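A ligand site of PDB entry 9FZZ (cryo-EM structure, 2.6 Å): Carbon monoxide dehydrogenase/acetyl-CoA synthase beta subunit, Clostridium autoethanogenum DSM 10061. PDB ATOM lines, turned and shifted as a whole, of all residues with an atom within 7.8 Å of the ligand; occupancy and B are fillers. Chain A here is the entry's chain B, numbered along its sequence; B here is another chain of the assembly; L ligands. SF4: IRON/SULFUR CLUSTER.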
ATOM      1  N   GLN A  36      15.322   3.378  32.064  1.00  0.00           N
ATOM      2  CA  GLN A  36      14.334   3.261  31.003  1.00  0.00           C
ATOM      3  C   GLN A  36      14.702   4.165  29.830  1.00  0.00           C
ATOM      4  O   GLN A  36      15.401   5.176  29.972  1.00  0.00           O
ATOM      5  CB  GLN A  36      12.941   3.570  31.564  1.00  0.00           C
ATOM      6  CG  GLN A  36      12.467   2.483  32.543  1.00  0.00           C
ATOM      7  CD  GLN A  36      11.108   2.805  33.167  1.00  0.00           C
ATOM      8  OE1 GLN A  36      10.967   3.770  33.905  1.00  0.00           O
ATOM      9  NE2 GLN A  36      10.094   1.986  32.861  1.00  0.00           N
ATOM     10  N   CYS A  37      14.199   3.793  28.647  1.00  0.00           N
ATOM     11  CA  CYS A  37      14.611   4.477  27.430  1.00  0.00           C
ATOM     12  C   CYS A  37      14.296   5.973  27.497  1.00  0.00           C
ATOM     13  O   CYS A  37      13.145   6.367  27.679  1.00  0.00           O
ATOM     14  CB  CYS A  37      13.929   3.852  26.208  1.00  0.00           C
ATOM     15  SG  CYS A  37      14.230   4.800  24.686  1.00  0.00           S
ATOM     16  N   GLY A  38      15.317   6.788  27.236  1.00  0.00           N
ATOM     17  CA  GLY A  38      15.141   8.230  27.290  1.00  0.00           C
ATOM     18  C   GLY A  38      14.183   8.755  26.247  1.00  0.00           C
ATOM     19  O   GLY A  38      13.377   9.641  26.529  1.00  0.00           O
ATOM     20  N   PHE A  39      14.230   8.186  25.026  1.00  0.00           N
ATOM     21  CA  PHE A  39      13.332   8.638  23.956  1.00  0.00           C
ATOM     22  C   PHE A  39      11.874   8.388  24.320  1.00  0.00           C
ATOM     23  O   PHE A  39      11.027   9.269  24.184  1.00  0.00           O
ATOM     24  CB  PHE A  39      13.666   7.929  22.636  1.00  0.00           C
ATOM     25  CG  PHE A  39      15.034   8.230  22.116  1.00  0.00           C
ATOM     26  CD1 PHE A  39      15.309   9.468  21.523  1.00  0.00           C
ATOM     27  CD2 PHE A  39      16.061   7.290  22.234  1.00  0.00           C
ATOM     28  CE1 PHE A  39      16.592   9.764  21.036  1.00  0.00           C
ATOM     29  CE2 PHE A  39      17.352   7.568  21.763  1.00  0.00           C
ATOM     30  CZ  PHE A  39      17.619   8.813  21.157  1.00  0.00           C
ATOM     31  N   GLY A  40      11.575   7.174  24.790  1.00  0.00           N
ATOM     32  CA  GLY A  40      10.218   6.868  25.209  1.00  0.00           C
ATOM     33  C   GLY A  40       9.781   7.672  26.422  1.00  0.00           C
ATOM     34  O   GLY A  40       8.617   8.062  26.541  1.00  0.00           O
ATOM     35  N   SER A  41      10.710   7.907  27.353  1.00  0.00           N
ATOM     36  CA  SER A  41      10.386   8.686  28.543  1.00  0.00           C
ATOM     37  C   SER A  41      10.029  10.131  28.173  1.00  0.00           C
ATOM     38  O   SER A  41       9.139  10.721  28.779  1.00  0.00           O
ATOM     39  CB  SER A  41      11.545   8.661  29.544  1.00  0.00           C
ATOM     40  OG  SER A  41      11.865   7.337  29.932  1.00  0.00           O
ATOM     41  N   ALA A  42      10.711  10.703  27.179  1.00  0.00           N
ATOM     42  CA  ALA A  42      10.408  12.056  26.744  1.00  0.00           C
ATOM     43  C   ALA A  42       9.263  12.117  25.726  1.00  0.00           C
ATOM     44  O   ALA A  42       8.790  13.215  25.420  1.00  0.00           O
ATOM     45  CB  ALA A  42      11.652  12.733  26.158  1.00  0.00           C
ATOM     46  N   GLY A  43       8.825  10.981  25.197  1.00  0.00           N
ATOM     47  CA  GLY A  43       7.750  10.955  24.228  1.00  0.00           C
ATOM     48  C   GLY A  43       8.149  11.300  22.806  1.00  0.00           C
ATOM     49  O   GLY A  43       7.273  11.572  21.980  1.00  0.00           O
ATOM     50  N   VAL A  44       9.446  11.286  22.492  1.00  0.00           N
ATOM     51  CA  VAL A  44       9.965  11.636  21.174  1.00  0.00           C
ATOM     52  C   VAL A  44      10.190  10.413  20.292  1.00  0.00           C
ATOM     53  O   VAL A  44      10.826  10.519  19.235  1.00  0.00           O
ATOM     54  CB  VAL A  44      11.228  12.495  21.259  1.00  0.00           C
ATOM     55  CG1 VAL A  44      10.863  13.937  21.635  1.00  0.00           C
ATOM     56  CG2 VAL A  44      12.248  11.905  22.263  1.00  0.00           C
ATOM     57  N   CYS A  45       9.717   9.242  20.712  1.00  0.00           N
ATOM     58  CA  CYS A  45       9.766   8.045  19.878  1.00  0.00           C
ATOM     59  C   CYS A  45       8.412   7.839  19.225  1.00  0.00           C
ATOM     60  O   CYS A  45       7.374   8.009  19.880  1.00  0.00           O
ATOM     61  CB  CYS A  45      10.130   6.801  20.697  1.00  0.00           C
ATOM     62  SG  CYS A  45       9.963   5.253  19.751  1.00  0.00           S
ATOM     63  N   CYS A  46       8.413   7.448  17.956  1.00  0.00           N
ATOM     64  CA  CYS A  46       7.187   7.205  17.232  1.00  0.00           C
ATOM     65  C   CYS A  46       7.238   5.842  16.565  1.00  0.00           C
ATOM     66  O   CYS A  46       8.267   5.427  16.043  1.00  0.00           O
ATOM     67  CB  CYS A  46       6.935   8.288  16.166  1.00  0.00           C
ATOM     68  SG  CYS A  46       5.327   8.086  15.361  1.00  0.00           S
ATOM     69  N   ARG A  47       6.107   5.128  16.613  1.00  0.00           N
ATOM     70  CA  ARG A  47       5.992   3.836  15.930  1.00  0.00           C
ATOM     71  C   ARG A  47       4.665   3.739  15.180  1.00  0.00           C
ATOM     72  O   ARG A  47       4.174   2.636  14.939  1.00  0.00           O
ATOM     73  CB  ARG A  47       6.138   2.670  16.913  1.00  0.00           C
ATOM     74  CG  ARG A  47       7.514   2.626  17.610  1.00  0.00           C
ATOM     75  CD  ARG A  47       7.756   1.267  18.299  1.00  0.00           C
ATOM     76  NE  ARG A  47       6.690   0.951  19.239  1.00  0.00           N
ATOM     77  CZ  ARG A  47       6.749   1.201  20.541  1.00  0.00           C
ATOM     78  NH1 ARG A  47       7.825   1.697  21.111  1.00  0.00           N
ATOM     79  NH2 ARG A  47       5.676   0.934  21.301  1.00  0.00           N
ATOM     80  N   PRO A  53      10.553   2.302  13.320  1.00  0.00           N
ATOM     81  CA  PRO A  53      10.453   3.318  14.412  1.00  0.00           C
ATOM     82  C   PRO A  53      11.327   4.551  14.206  1.00  0.00           C
ATOM     83  O   PRO A  53      12.431   4.455  13.706  1.00  0.00           O
ATOM     84  CB  PRO A  53      10.929   2.544  15.674  1.00  0.00           C
ATOM     85  CG  PRO A  53      10.991   1.072  15.283  1.00  0.00           C
ATOM     86  CD  PRO A  53      11.231   1.071  13.785  1.00  0.00           C
ATOM     87  N   CYS A  54      10.807   5.738  14.588  1.00  0.00           N
ATOM     88  CA  CYS A  54      11.537   6.999  14.494  1.00  0.00           C
ATOM     89  C   CYS A  54      11.722   7.571  15.894  1.00  0.00           C
ATOM     90  O   CYS A  54      10.779   7.585  16.702  1.00  0.00           O
ATOM     91  CB  CYS A  54      10.808   8.040  13.615  1.00  0.00           C
ATOM     92  SG  CYS A  54      10.654   7.626  11.858  1.00  0.00           S
ATOM     93  N   ARG A  55      12.921   8.030  16.177  1.00  0.00           N
ATOM     94  CA  ARG A  55      13.216   8.766  17.391  1.00  0.00           C
ATOM     95  C   ARG A  55      13.914  10.059  16.996  1.00  0.00           C
ATOM     96  O   ARG A  55      14.848  10.056  16.184  1.00  0.00           O
ATOM     97  CB  ARG A  55      14.056   7.946  18.371  1.00  0.00           C
ATOM     98  CG  ARG A  55      15.200   7.190  17.761  1.00  0.00           C
ATOM     99  CD  ARG A  55      15.715   6.151  18.751  1.00  0.00           C
ATOM    100  NE  ARG A  55      16.827   5.424  18.162  1.00  0.00           N
ATOM    101  CZ  ARG A  55      17.378   4.311  18.646  1.00  0.00           C
ATOM    102  NH1 ARG A  55      16.916   3.747  19.743  1.00  0.00           N
ATOM    103  NH2 ARG A  55      18.406   3.763  18.002  1.00  0.00           N
ATOM    104  N   GLN B  36      17.538   1.802  12.959  1.00  0.00           N
ATOM    105  CA  GLN B  36      16.346   2.039  13.757  1.00  0.00           C
ATOM    106  C   GLN B  36      16.324   1.120  14.981  1.00  0.00           C
ATOM    107  O   GLN B  36      16.933   0.043  14.996  1.00  0.00           O
ATOM    108  CB  GLN B  36      15.089   1.869  12.898  1.00  0.00           C
ATOM    109  CG  GLN B  36      14.937   2.992  11.864  1.00  0.00           C
ATOM    110  CD  GLN B  36      13.737   2.778  10.929  1.00  0.00           C
ATOM    111  OE1 GLN B  36      13.681   1.784  10.219  1.00  0.00           O
ATOM    112  NE2 GLN B  36      12.783   3.705  10.946  1.00  0.00           N
ATOM    113  N   CYS B  37      15.608   1.551  16.009  1.00  0.00           N
ATOM    114  CA  CYS B  37      15.652   0.844  17.280  1.00  0.00           C
ATOM    115  C   CYS B  37      15.214  -0.604  17.120  1.00  0.00           C
ATOM    116  O   CYS B  37      14.095  -0.883  16.667  1.00  0.00           O
ATOM    117  CB  CYS B  37      14.768   1.558  18.312  1.00  0.00           C
ATOM    118  SG  CYS B  37      14.615   0.593  19.855  1.00  0.00           S
ATOM    119  N   GLY B  38      16.048  -1.523  17.606  1.00  0.00           N
ATOM    120  CA  GLY B  38      15.748  -2.930  17.493  1.00  0.00           C
ATOM    121  C   GLY B  38      14.523  -3.355  18.277  1.00  0.00           C
ATOM    122  O   GLY B  38      13.722  -4.169  17.805  1.00  0.00           O
ATOM    123  N   PHE B  39      14.338  -2.779  19.481  1.00  0.00           N
ATOM    124  CA  PHE B  39      13.174  -3.129  20.294  1.00  0.00           C
ATOM    125  C   PHE B  39      11.874  -2.749  19.604  1.00  0.00           C
ATOM    126  O   PHE B  39      10.936  -3.551  19.519  1.00  0.00           O
ATOM    127  CB  PHE B  39      13.245  -2.448  21.675  1.00  0.00           C
ATOM    128  CG  PHE B  39      14.415  -2.866  22.507  1.00  0.00           C
ATOM    129  CD1 PHE B  39      14.417  -4.103  23.150  1.00  0.00           C
ATOM    130  CD2 PHE B  39      15.510  -2.020  22.650  1.00  0.00           C
ATOM    131  CE1 PHE B  39      15.513  -4.507  23.928  1.00  0.00           C
ATOM    132  CE2 PHE B  39      16.628  -2.406  23.426  1.00  0.00           C
ATOM    133  CZ  PHE B  39      16.628  -3.663  24.074  1.00  0.00           C
ATOM    134  N   GLY B  40      11.807  -1.516  19.090  1.00  0.00           N
ATOM    135  CA  GLY B  40      10.623  -1.089  18.379  1.00  0.00           C
ATOM    136  C   GLY B  40      10.418  -1.843  17.075  1.00  0.00           C
ATOM    137  O   GLY B  40       9.281  -2.117  16.680  1.00  0.00           O
ATOM    138  N   SER B  41      11.511  -2.190  16.387  1.00  0.00           N
ATOM    139  CA  SER B  41      11.389  -2.947  15.144  1.00  0.00           C
ATOM    140  C   SER B  41      10.824  -4.336  15.402  1.00  0.00           C
ATOM    141  O   SER B  41      10.037  -4.851  14.597  1.00  0.00           O
ATOM    142  CB  SER B  41      12.749  -3.050  14.445  1.00  0.00           C
ATOM    143  OG  SER B  41      13.281  -1.768  14.159  1.00  0.00           O
ATOM    144  N   ALA B  42      11.194  -4.973  16.514  1.00  0.00           N
ATOM    145  CA  ALA B  42      10.662  -6.281  16.859  1.00  0.00           C
ATOM    146  C   ALA B  42       9.319  -6.216  17.580  1.00  0.00           C
ATOM    147  O   ALA B  42       8.672  -7.260  17.742  1.00  0.00           O
ATOM    148  CB  ALA B  42      11.670  -7.072  17.715  1.00  0.00           C
ATOM    149  N   GLY B  43       8.874  -5.035  18.002  1.00  0.00           N
ATOM    150  CA  GLY B  43       7.608  -4.888  18.701  1.00  0.00           C
ATOM    151  C   GLY B  43       7.626  -5.257  20.164  1.00  0.00           C
ATOM    152  O   GLY B  43       6.558  -5.440  20.759  1.00  0.00           O
ATOM    153  N   VAL B  44       8.808  -5.356  20.782  1.00  0.00           N
ATOM    154  CA  VAL B  44       8.963  -5.751  22.183  1.00  0.00           C
ATOM    155  C   VAL B  44       9.106  -4.537  23.106  1.00  0.00           C
ATOM    156  O   VAL B  44       9.461  -4.692  24.282  1.00  0.00           O
ATOM    157  CB  VAL B  44      10.120  -6.735  22.378  1.00  0.00           C
ATOM    158  CG1 VAL B  44       9.701  -8.134  21.918  1.00  0.00           C
ATOM    159  CG2 VAL B  44      11.401  -6.260  21.649  1.00  0.00           C
ATOM    160  N   CYS B  45       8.855  -3.329  22.599  1.00  0.00           N
ATOM    161  CA  CYS B  45       8.826  -2.135  23.426  1.00  0.00           C
ATOM    162  C   CYS B  45       7.384  -1.788  23.744  1.00  0.00           C
ATOM    163  O   CYS B  45       6.516  -1.868  22.873  1.00  0.00           O
ATOM    164  CB  CYS B  45       9.493  -0.940  22.741  1.00  0.00           C
ATOM    165  SG  CYS B  45       9.263   0.627  23.638  1.00  0.00           S
ATOM    166  N   CYS B  46       7.124  -1.393  24.985  1.00  0.00           N
ATOM    167  CA  CYS B  46       5.793  -1.011  25.400  1.00  0.00           C
ATOM    168  C   CYS B  46       5.812   0.359  26.074  1.00  0.00           C
ATOM    169  O   CYS B  46       6.735   0.665  26.831  1.00  0.00           O
ATOM    170  CB  CYS B  46       5.190  -2.048  26.374  1.00  0.00           C
ATOM    171  SG  CYS B  46       3.468  -1.692  26.764  1.00  0.00           S
ATOM    172  N   ARG B  47       4.810   1.171  25.773  1.00  0.00           N
ATOM    173  CA  ARG B  47       4.667   2.476  26.425  1.00  0.00           C
ATOM    174  C   ARG B  47       3.218   2.713  26.842  1.00  0.00           C
ATOM    175  O   ARG B  47       2.795   3.865  26.984  1.00  0.00           O
ATOM    176  CB  ARG B  47       5.156   3.610  25.518  1.00  0.00           C
ATOM    177  CG  ARG B  47       6.645   3.499  25.166  1.00  0.00           C
ATOM    178  CD  ARG B  47       7.185   4.820  24.580  1.00  0.00           C
ATOM    179  NE  ARG B  47       6.409   5.237  23.408  1.00  0.00           N
ATOM    180  CZ  ARG B  47       6.726   4.959  22.154  1.00  0.00           C
ATOM    181  NH1 ARG B  47       7.851   4.341  21.849  1.00  0.00           N
ATOM    182  NH2 ARG B  47       5.894   5.324  21.175  1.00  0.00           N
ATOM    183  N   PRO B  53       8.614   3.569  30.055  1.00  0.00           N
ATOM    184  CA  PRO B  53       8.675   2.565  28.956  1.00  0.00           C
ATOM    185  C   PRO B  53       9.338   1.245  29.348  1.00  0.00           C
ATOM    186  O   PRO B  53      10.296   1.236  30.096  1.00  0.00           O
ATOM    187  CB  PRO B  53       9.507   3.275  27.861  1.00  0.00           C
ATOM    188  CG  PRO B  53       9.632   4.740  28.283  1.00  0.00           C
ATOM    189  CD  PRO B  53       9.502   4.724  29.787  1.00  0.00           C
ATOM    190  N   CYS B  54       8.806   0.123  28.848  1.00  0.00           N
ATOM    191  CA  CYS B  54       9.366  -1.206  29.086  1.00  0.00           C
ATOM    192  C   CYS B  54       9.814  -1.818  27.774  1.00  0.00           C
ATOM    193  O   CYS B  54       9.102  -1.738  26.766  1.00  0.00           O
ATOM    194  CB  CYS B  54       8.359  -2.157  29.767  1.00  0.00           C
ATOM    195  SG  CYS B  54       7.839  -1.711  31.434  1.00  0.00           S
ATOM    196  N   ARG B  55      11.006  -2.378  27.773  1.00  0.00           N
ATOM    197  CA  ARG B  55      11.504  -3.154  26.653  1.00  0.00           C
ATOM    198  C   ARG B  55      11.957  -4.506  27.186  1.00  0.00           C
ATOM    199  O   ARG B  55      12.670  -4.588  28.185  1.00  0.00           O
ATOM    200  CB  ARG B  55      12.618  -2.433  25.907  1.00  0.00           C
ATOM    201  CG  ARG B  55      13.656  -1.788  26.778  1.00  0.00           C
ATOM    202  CD  ARG B  55      14.490  -0.817  25.950  1.00  0.00           C
ATOM    203  NE  ARG B  55      15.489  -0.185  26.799  1.00  0.00           N
ATOM    204  CZ  ARG B  55      16.238   0.860  26.461  1.00  0.00           C
ATOM    205  NH1 ARG B  55      16.126   1.441  25.287  1.00  0.00           N
ATOM    206  NH2 ARG B  55      17.114   1.336  27.347  1.00  0.00           N
HETATM  207 FE1  SF4 L   1      13.012   3.688  23.104  1.00  0.00          FE
HETATM  208 FE2  SF4 L   1      11.010   1.851  22.792  1.00  0.00          FE
HETATM  209 FE3  SF4 L   1      13.157   1.827  21.099  1.00  0.00          FE
HETATM  210 FE4  SF4 L   1      11.331   3.857  20.954  1.00  0.00          FE
HETATM  211  S1  SF4 L   1      10.969   1.643  20.518  1.00  0.00           S
HETATM  212  S2  SF4 L   1      13.595   4.059  20.917  1.00  0.00           S
HETATM  213  S3  SF4 L   1      10.777   4.095  23.156  1.00  0.00           S
HETATM  214  S4  SF4 L   1      13.179   1.424  23.359  1.00  0.00           S
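SG of Cys 37 of chain B binds FE3 of the ligand (2.3 Å). The side-chain sulfur (SG) of Cys 37 of chain A is bound to an iron atom (FE1) of the ligand (2.3 Å). The side-chain sulfur of Cys 45 of chain B binds an iron atom (FE2) of the ligand (2.3 Å). SG of Cys 45 of chain A binds FE4 of the ligand, 2.3 Å away. The guanidinium group (NH1) of Arg 47 of chain A sits close to a sulfur (S1) of the ligand. NH1 of Arg 47 of chain B sits close to S3 of the ligand, at 3.2 Å. The backbone NH of Gly 40 of chain B sits close to a sulfur (S1) of the ligand (3.6 Å). The backbone NH (N) of Gly 40 of chain A sits close to a sulfur (S3) of the ligand (3.6 Å). NH1 of Arg 55 of chain B lies close to S4 of the ligand (3.5 Å). S2 of the ligand sits close to NH1 of Arg 55 of chain A (3.5 Å).
The backbone NH of Gly 40 of chain B lies close to the side-chain sulfur of Cys 37 of chain B, 3.6 Å away. SG of Cys 37 of chain B sits close to N of Phe 39 of chain B. The side-chain sulfur of Cys 37 of chain A sits close to the backbone NH of Gly 40 of chain A. The side-chain sulfur (SG) of Cys 37 of chain A sits close to the backbone NH (N) of Phe 39 of chain A, 3.4 Å away. The side-chain hydroxyl (OG) of Ser 41 of chain A sits at hydrogen-bond distance from the backbone carbonyl oxygen (O) of Cys 37 of chain A (2.8 Å). O of Cys 45 of chain B sits at hydrogen-bond distance from NH2 of Arg 47 of chain A (3.3 Å). The backbone carbonyl oxygen (O) of Cys 45 of chain A sits at hydrogen-bond distance from the guanidinium group (NH2) of Arg 47 of chain B, at 3.3 Å. The guanidinium group (NH1) of Arg 47 of chain A lies close to the guanidinium group (NH1) of Arg 47 of chain B (2.7 Å).
Ten residues have an atom within 4 Å of the ligand: Cys 37 of chain A, Gly 40 of chain A, Cys 45 of chain A, Arg 47 of chain A, Arg 55 of chain A, Cys 37 of chain B, Gly 40 of chain B, Cys 45 of chain B, Arg 47 of chain B and Arg 55 of chain B. The nearest printed residue that does not touch the ligand is Phe 39 of chain B (4.2 Å).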
